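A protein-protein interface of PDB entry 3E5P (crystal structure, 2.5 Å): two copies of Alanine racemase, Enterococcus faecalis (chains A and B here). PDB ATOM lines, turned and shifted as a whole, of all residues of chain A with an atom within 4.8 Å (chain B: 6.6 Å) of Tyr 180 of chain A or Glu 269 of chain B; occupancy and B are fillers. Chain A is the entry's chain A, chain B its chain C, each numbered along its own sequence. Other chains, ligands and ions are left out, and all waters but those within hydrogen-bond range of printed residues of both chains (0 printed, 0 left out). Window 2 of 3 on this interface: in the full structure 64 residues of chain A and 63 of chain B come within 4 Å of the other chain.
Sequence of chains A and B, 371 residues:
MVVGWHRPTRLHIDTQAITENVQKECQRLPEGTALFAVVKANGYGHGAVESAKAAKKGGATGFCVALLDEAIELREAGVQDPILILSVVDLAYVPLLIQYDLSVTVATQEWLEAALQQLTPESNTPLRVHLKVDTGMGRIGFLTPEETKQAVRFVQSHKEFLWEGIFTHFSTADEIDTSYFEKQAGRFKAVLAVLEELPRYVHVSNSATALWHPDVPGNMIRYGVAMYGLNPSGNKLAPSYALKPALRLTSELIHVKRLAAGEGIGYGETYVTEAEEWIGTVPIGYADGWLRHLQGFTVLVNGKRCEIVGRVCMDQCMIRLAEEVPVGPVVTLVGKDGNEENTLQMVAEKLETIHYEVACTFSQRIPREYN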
ATOM      1  N   GLY A 136     -16.432  -9.456  -7.468  1.00  0.00           N
ATOM      2  CA  GLY A 136     -16.326  -8.272  -6.632  1.00  0.00           C
ATOM      3  C   GLY A 136     -17.096  -7.027  -7.017  1.00  0.00           C
ATOM      4  O   GLY A 136     -17.718  -6.413  -6.158  1.00  0.00           O
ATOM      5  N   MET A 137     -17.047  -6.636  -8.289  1.00  0.00           N
ATOM      6  CA  MET A 137     -17.757  -5.440  -8.752  1.00  0.00           C
ATOM      7  C   MET A 137     -19.182  -5.427  -8.214  1.00  0.00           C
ATOM      8  O   MET A 137     -19.648  -4.416  -7.695  1.00  0.00           O
ATOM      9  CB  MET A 137     -17.784  -5.387 -10.282  1.00  0.00           C
ATOM     10  CG  MET A 137     -18.394  -4.120 -10.868  1.00  0.00           C
ATOM     11  SD  MET A 137     -17.456  -2.622 -10.499  1.00  0.00           S
ATOM     12  CE  MET A 137     -18.701  -1.335 -10.737  1.00  0.00           C
ATOM     13  N   SER A 171     -12.891  -3.334  -9.191  1.00  0.00           N
ATOM     14  CA  SER A 171     -13.595  -2.127  -8.762  1.00  0.00           C
ATOM     15  C   SER A 171     -12.746  -1.129  -7.994  1.00  0.00           C
ATOM     16  O   SER A 171     -13.144   0.020  -7.819  1.00  0.00           O
ATOM     17  CB  SER A 171     -14.782  -2.497  -7.886  1.00  0.00           C
ATOM     18  OG  SER A 171     -14.319  -3.009  -6.650  1.00  0.00           O
ATOM     19  N   THR A 172     -11.580  -1.561  -7.533  1.00  0.00           N
ATOM     20  CA  THR A 172     -10.721  -0.680  -6.750  1.00  0.00           C
ATOM     21  C   THR A 172      -9.262  -0.768  -7.148  1.00  0.00           C
ATOM     22  O   THR A 172      -8.387  -0.611  -6.303  1.00  0.00           O
ATOM     23  CB  THR A 172     -10.839  -1.012  -5.247  1.00  0.00           C
ATOM     24  OG1 THR A 172     -10.384  -2.346  -5.020  1.00  0.00           O
ATOM     25  CG2 THR A 172     -12.292  -0.924  -4.792  1.00  0.00           C
ATOM     26  N   THR A 178      -4.519  -1.878  -1.742  1.00  0.00           N
ATOM     27  CA  THR A 178      -4.709  -2.910  -2.748  1.00  0.00           C
ATOM     28  C   THR A 178      -5.423  -4.141  -2.209  1.00  0.00           C
ATOM     29  O   THR A 178      -5.525  -5.163  -2.884  1.00  0.00           O
ATOM     30  CB  THR A 178      -3.355  -3.330  -3.331  1.00  0.00           C
ATOM     31  OG1 THR A 178      -2.578  -3.974  -2.319  1.00  0.00           O
ATOM     32  CG2 THR A 178      -2.595  -2.115  -3.819  1.00  0.00           C
ATOM     33  N   SER A 179      -5.927  -4.023  -0.990  1.00  0.00           N
ATOM     34  CA  SER A 179      -6.627  -5.107  -0.321  1.00  0.00           C
ATOM     35  C   SER A 179      -7.724  -5.784  -1.167  1.00  0.00           C
ATOM     36  O   SER A 179      -7.556  -6.911  -1.651  1.00  0.00           O
ATOM     37  CB  SER A 179      -7.220  -4.562   0.975  1.00  0.00           C
ATOM     38  OG  SER A 179      -7.852  -5.584   1.711  1.00  0.00           O
ATOM     39  N   TYR A 180      -8.847  -5.092  -1.337  1.00  0.00           N
ATOM     40  CA  TYR A 180      -9.964  -5.626  -2.098  1.00  0.00           C
ATOM     41  C   TYR A 180      -9.579  -6.037  -3.514  1.00  0.00           C
ATOM     42  O   TYR A 180     -10.246  -6.859  -4.125  1.00  0.00           O
ATOM     43  CB  TYR A 180     -11.095  -4.606  -2.142  1.00  0.00           C
ATOM     44  CG  TYR A 180     -12.409  -5.162  -2.652  1.00  0.00           C
ATOM     45  CD1 TYR A 180     -12.922  -6.361  -2.155  1.00  0.00           C
ATOM     46  CD2 TYR A 180     -13.171  -4.461  -3.585  1.00  0.00           C
ATOM     47  CE1 TYR A 180     -14.166  -6.846  -2.570  1.00  0.00           C
ATOM     48  CE2 TYR A 180     -14.417  -4.937  -4.007  1.00  0.00           C
ATOM     49  CZ  TYR A 180     -14.910  -6.126  -3.493  1.00  0.00           C
ATOM     50  OH  TYR A 180     -16.153  -6.577  -3.882  1.00  0.00           O
ATOM     51  N   PHE A 181      -8.504  -5.461  -4.037  1.00  0.00           N
ATOM     52  CA  PHE A 181      -8.051  -5.795  -5.381  1.00  0.00           C
ATOM     53  C   PHE A 181      -7.546  -7.232  -5.421  1.00  0.00           C
ATOM     54  O   PHE A 181      -7.855  -7.989  -6.344  1.00  0.00           O
ATOM     55  CB  PHE A 181      -6.920  -4.863  -5.821  1.00  0.00           C
ATOM     56  CG  PHE A 181      -6.318  -5.238  -7.144  1.00  0.00           C
ATOM     57  CD1 PHE A 181      -6.841  -4.741  -8.325  1.00  0.00           C
ATOM     58  CD2 PHE A 181      -5.253  -6.121  -7.208  1.00  0.00           C
ATOM     59  CE1 PHE A 181      -6.314  -5.119  -9.556  1.00  0.00           C
ATOM     60  CE2 PHE A 181      -4.717  -6.507  -8.427  1.00  0.00           C
ATOM     61  CZ  PHE A 181      -5.248  -6.005  -9.606  1.00  0.00           C
ATOM     62  N   GLU A 182      -6.750  -7.597  -4.423  1.00  0.00           N
ATOM     63  CA  GLU A 182      -6.209  -8.944  -4.341  1.00  0.00           C
ATOM     64  C   GLU A 182      -7.331  -9.972  -4.216  1.00  0.00           C
ATOM     65  O   GLU A 182      -7.299 -11.014  -4.871  1.00  0.00           O
ATOM     66  CB  GLU A 182      -5.232  -9.038  -3.167  1.00  0.00           C
ATOM     67  CG  GLU A 182      -3.799  -8.677  -3.568  1.00  0.00           C
ATOM     68  CD  GLU A 182      -2.895  -8.264  -2.406  1.00  0.00           C
ATOM     69  OE1 GLU A 182      -2.800  -9.001  -1.395  1.00  0.00           O
ATOM     70  OE2 GLU A 182      -2.260  -7.193  -2.521  1.00  0.00           O
ATOM     71  N   LYS A 183      -8.338  -9.672  -3.399  1.00  0.00           N
ATOM     72  CA  LYS A 183      -9.464 -10.589  -3.235  1.00  0.00           C
ATOM     73  C   LYS A 183     -10.051 -10.946  -4.606  1.00  0.00           C
ATOM     74  O   LYS A 183     -10.152 -12.123  -4.967  1.00  0.00           O
ATOM     75  CB  LYS A 183     -10.564  -9.957  -2.374  1.00  0.00           C
ATOM     76  CG  LYS A 183     -10.124  -9.493  -0.993  1.00  0.00           C
ATOM     77  CD  LYS A 183     -11.259  -8.741  -0.281  1.00  0.00           C
ATOM     78  CE  LYS A 183     -10.771  -8.000   0.978  1.00  0.00           C
ATOM     79  NZ  LYS A 183     -11.844  -7.154   1.611  1.00  0.00           N
ATOM     80  N   GLN A 184     -10.435  -9.926  -5.369  1.00  0.00           N
ATOM     81  CA  GLN A 184     -11.017 -10.156  -6.686  1.00  0.00           C
ATOM     82  C   GLN A 184     -10.089 -10.992  -7.550  1.00  0.00           C
ATOM     83  O   GLN A 184     -10.525 -11.933  -8.213  1.00  0.00           O
ATOM     84  CB  GLN A 184     -11.327  -8.829  -7.394  1.00  0.00           C
ATOM     85  CG  GLN A 184     -12.410  -8.001  -6.717  1.00  0.00           C
ATOM     86  CD  GLN A 184     -12.952  -6.912  -7.619  1.00  0.00           C
ATOM     87  OE1 GLN A 184     -13.495  -7.195  -8.686  1.00  0.00           O
ATOM     88  NE2 GLN A 184     -12.809  -5.662  -7.198  1.00  0.00           N
ATOM     89  N   GLY B 262     -22.258  -8.735   3.429  1.00  0.00           N
ATOM     90  CA  GLY B 262     -20.826  -8.482   3.423  1.00  0.00           C
ATOM     91  C   GLY B 262     -20.151  -8.299   2.072  1.00  0.00           C
ATOM     92  O   GLY B 262     -18.925  -8.152   2.010  1.00  0.00           O
ATOM     93  N   GLU B 263     -20.923  -8.310   0.990  1.00  0.00           N
ATOM     94  CA  GLU B 263     -20.335  -8.136  -0.331  1.00  0.00           C
ATOM     95  C   GLU B 263     -20.331  -6.678  -0.761  1.00  0.00           C
ATOM     96  O   GLU B 263     -21.309  -5.952  -0.567  1.00  0.00           O
ATOM     97  CB  GLU B 263     -21.071  -8.986  -1.368  1.00  0.00           C
ATOM     98  CG  GLU B 263     -20.684 -10.456  -1.349  1.00  0.00           C
ATOM     99  CD  GLU B 263     -19.201 -10.683  -1.639  1.00  0.00           C
ATOM    100  OE1 GLU B 263     -18.794 -11.859  -1.754  1.00  0.00           O
ATOM    101  OE2 GLU B 263     -18.439  -9.696  -1.751  1.00  0.00           O
ATOM    102  N   GLY B 264     -19.208  -6.253  -1.331  1.00  0.00           N
ATOM    103  CA  GLY B 264     -19.071  -4.881  -1.787  1.00  0.00           C
ATOM    104  C   GLY B 264     -19.569  -4.753  -3.207  1.00  0.00           C
ATOM    105  O   GLY B 264     -19.441  -5.688  -3.993  1.00  0.00           O
ATOM    106  N   ILE B 265     -20.157  -3.609  -3.538  1.00  0.00           N
ATOM    107  CA  ILE B 265     -20.662  -3.401  -4.886  1.00  0.00           C
ATOM    108  C   ILE B 265     -20.313  -2.013  -5.446  1.00  0.00           C
ATOM    109  O   ILE B 265     -20.412  -0.990  -4.756  1.00  0.00           O
ATOM    110  CB  ILE B 265     -22.206  -3.643  -4.951  1.00  0.00           C
ATOM    111  CG1 ILE B 265     -22.977  -2.466  -4.380  1.00  0.00           C
ATOM    112  CG2 ILE B 265     -22.579  -4.857  -4.115  1.00  0.00           C
ATOM    113  CD1 ILE B 265     -24.459  -2.610  -4.581  1.00  0.00           C
ATOM    114  N   GLY B 266     -19.877  -1.993  -6.700  1.00  0.00           N
ATOM    115  CA  GLY B 266     -19.519  -0.738  -7.333  1.00  0.00           C
ATOM    116  C   GLY B 266     -18.064  -0.358  -7.138  1.00  0.00           C
ATOM    117  O   GLY B 266     -17.322  -1.042  -6.426  1.00  0.00           O
ATOM    118  N   TYR B 267     -17.657   0.735  -7.778  1.00  0.00           N
ATOM    119  CA  TYR B 267     -16.285   1.224  -7.682  1.00  0.00           C
ATOM    120  C   TYR B 267     -15.979   1.718  -6.276  1.00  0.00           C
ATOM    121  O   TYR B 267     -16.842   2.295  -5.613  1.00  0.00           O
ATOM    122  CB  TYR B 267     -16.055   2.362  -8.676  1.00  0.00           C
ATOM    123  CG  TYR B 267     -15.925   1.919 -10.104  1.00  0.00           C
ATOM    124  CD1 TYR B 267     -14.928   1.029 -10.484  1.00  0.00           C
ATOM    125  CD2 TYR B 267     -16.776   2.415 -11.086  1.00  0.00           C
ATOM    126  CE1 TYR B 267     -14.779   0.646 -11.810  1.00  0.00           C
ATOM    127  CE2 TYR B 267     -16.635   2.036 -12.417  1.00  0.00           C
ATOM    128  CZ  TYR B 267     -15.634   1.151 -12.768  1.00  0.00           C
ATOM    129  OH  TYR B 267     -15.494   0.758 -14.073  1.00  0.00           O
ATOM    130  N   GLY B 268     -14.746   1.492  -5.832  1.00  0.00           N
ATOM    131  CA  GLY B 268     -14.341   1.918  -4.504  1.00  0.00           C
ATOM    132  C   GLY B 268     -15.048   1.167  -3.389  1.00  0.00           C
ATOM    133  O   GLY B 268     -14.763   1.375  -2.208  1.00  0.00           O
ATOM    134  N   GLU B 269     -15.960   0.276  -3.767  1.00  0.00           N
ATOM    135  CA  GLU B 269     -16.726  -0.497  -2.801  1.00  0.00           C
ATOM    136  C   GLU B 269     -17.325   0.465  -1.783  1.00  0.00           C
ATOM    137  O   GLU B 269     -17.116   0.321  -0.576  1.00  0.00           O
ATOM    138  CB  GLU B 269     -15.835  -1.509  -2.080  1.00  0.00           C
ATOM    139  CG  GLU B 269     -16.632  -2.536  -1.290  1.00  0.00           C
ATOM    140  CD  GLU B 269     -15.779  -3.399  -0.366  1.00  0.00           C
ATOM    141  OE1 GLU B 269     -16.315  -4.408   0.157  1.00  0.00           O
ATOM    142  OE2 GLU B 269     -14.586  -3.069  -0.159  1.00  0.00           O
ATOM    143  N   THR B 270     -18.062   1.456  -2.275  1.00  0.00           N
ATOM    144  CA  THR B 270     -18.679   2.434  -1.394  1.00  0.00           C
ATOM    145  C   THR B 270     -19.846   1.799  -0.656  1.00  0.00           C
ATOM    146  O   THR B 270     -20.246   2.271   0.404  1.00  0.00           O
ATOM    147  CB  THR B 270     -19.203   3.644  -2.178  1.00  0.00           C
ATOM    148  OG1 THR B 270     -20.321   3.244  -2.974  1.00  0.00           O
ATOM    149  CG2 THR B 270     -18.121   4.206  -3.073  1.00  0.00           C
ATOM    150  N   TYR B 271     -20.383   0.723  -1.222  1.00  0.00           N
ATOM    151  CA  TYR B 271     -21.507   0.015  -0.619  1.00  0.00           C
ATOM    152  C   TYR B 271     -21.208  -1.462  -0.307  1.00  0.00           C
ATOM    153  O   TYR B 271     -20.563  -2.158  -1.097  1.00  0.00           O
ATOM    154  CB  TYR B 271     -22.717   0.076  -1.547  1.00  0.00           C
ATOM    155  CG  TYR B 271     -23.971  -0.528  -0.951  1.00  0.00           C
ATOM    156  CD1 TYR B 271     -24.668   0.131   0.067  1.00  0.00           C
ATOM    157  CD2 TYR B 271     -24.458  -1.763  -1.394  1.00  0.00           C
ATOM    158  CE1 TYR B 271     -25.817  -0.421   0.627  1.00  0.00           C
ATOM    159  CE2 TYR B 271     -25.607  -2.327  -0.840  1.00  0.00           C
ATOM    160  CZ  TYR B 271     -26.283  -1.646   0.172  1.00  0.00           C
ATOM    161  OH  TYR B 271     -27.424  -2.179   0.727  1.00  0.00           O
ATOM    162  N   VAL B 272     -21.679  -1.929   0.849  1.00  0.00           N
ATOM    163  CA  VAL B 272     -21.508  -3.326   1.247  1.00  0.00           C
ATOM    164  C   VAL B 272     -22.839  -3.887   1.748  1.00  0.00           C
ATOM    165  O   VAL B 272     -23.503  -3.287   2.603  1.00  0.00           O
ATOM    166  CB  VAL B 272     -20.439  -3.503   2.360  1.00  0.00           C
ATOM    167  CG1 VAL B 272     -19.076  -3.069   1.845  1.00  0.00           C
ATOM    168  CG2 VAL B 272     -20.828  -2.714   3.602  1.00  0.00           C
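The backbone NH (N) of Gly 268 of chain B is in hydrogen-bond range of the backbone carbonyl oxygen (O) of Ser 171 of chain A (2.9 Å).
The backbone carbonyl oxygen (O) of Met 137 of chain A lies within hydrogen-bond range of the backbone NH (N) of Gly 266 of chain B.
OH of Tyr 180 of chain A sits at hydrogen-bond distance from O of Gly 264 of chain B, at 3.4 Å.
The backbone carbonyl oxygen (O) of Gly 264 of chain B sits close to the backbone carbonyl oxygen (O) of Gly 136 of chain A (2.9 Å).
N of Ile 265 of chain B sits at hydrogen-bond distance from O of Tyr 271 of chain B (2.9 Å).
The side-chain hydroxyl (OH) of Tyr 180 of chain A lies within hydrogen-bond range of the backbone carbonyl oxygen (O) of Gly 136 of chain A (2.8 Å).
The backbone NH of Ser 171 of chain A lies close to the side-chain amide nitrogen of Gln 184 of chain A (3.1 Å).
Among the printed residues, merely in contact across the chains: Met 137 of chain A with Ile 265 of chain B (3.2 Å), Ser 171 of chain A with Gly 266 of chain B (3.3 Å), Ser 171 of chain A with Tyr 267 of chain B (3.4 Å), Thr 172 of chain A with Gly 268 of chain B (3.5 Å), Met 137 of chain A with Tyr 267 of chain B (3.8 Å), Tyr 180 of chain A with Glu 269 of chain B (3.9 Å), Met 137 of chain A with Gly 264 of chain B (3.9 Å) and Thr 172 of chain A with Glu 269 of chain B (3.99 Å).
Printed residues of chain A within 4 Å of Glu 269 of chain B: Thr 172 (3.99 Å) and Tyr 180 (3.9 Å).
Printed residues of chain B within 4 Å of Ser 171 of chain A: Gly 266 (3.3 Å), Tyr 267 (3.4 Å) and Gly 268 (2.9 Å).
Printed residues of chain A within 4 Å of Tyr 267 of chain B: Met 137 (3.8 Å) and Ser 171 (3.4 Å).
Of the printed residues of chain A, Gly 266 of chain B touches Met 137 (2.6 Å) and Ser 171 (3.3 Å).
Of the printed residues of chain B, Thr 172 of chain A touches Gly 268 (3.5 Å) and Glu 269 (3.99 Å).
Printed residues of chain A within 4 Å of Gly 264 of chain B: Gly 136 (2.9 Å), Met 137 (3.9 Å) and Tyr 180 (3.4 Å).
Glu 263 of chain B touches none of the printed residues of chain A.
Phe 181 of chain A touches none of the printed residues of chain B.
The nearest residue of chain B that does not touch Tyr 180 of chain A is Glu 263 of chain B (4.4 Å).
The nearest printed residue of chain B that does not touch Met 137 of chain A is Gly 268 of chain B (6.8 Å).
Among the printed residues, 12 pairs touch across the chains.
Among the printed residues, no Asp or Glu carboxylate lies within 4 Å of a Lys or Arg side-chain nitrogen of the other chain.
No position is printed for both chains.
Of the 12 pairs that touch across the chains among the printed residues, none has its exchanged pair printed and touching as well.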
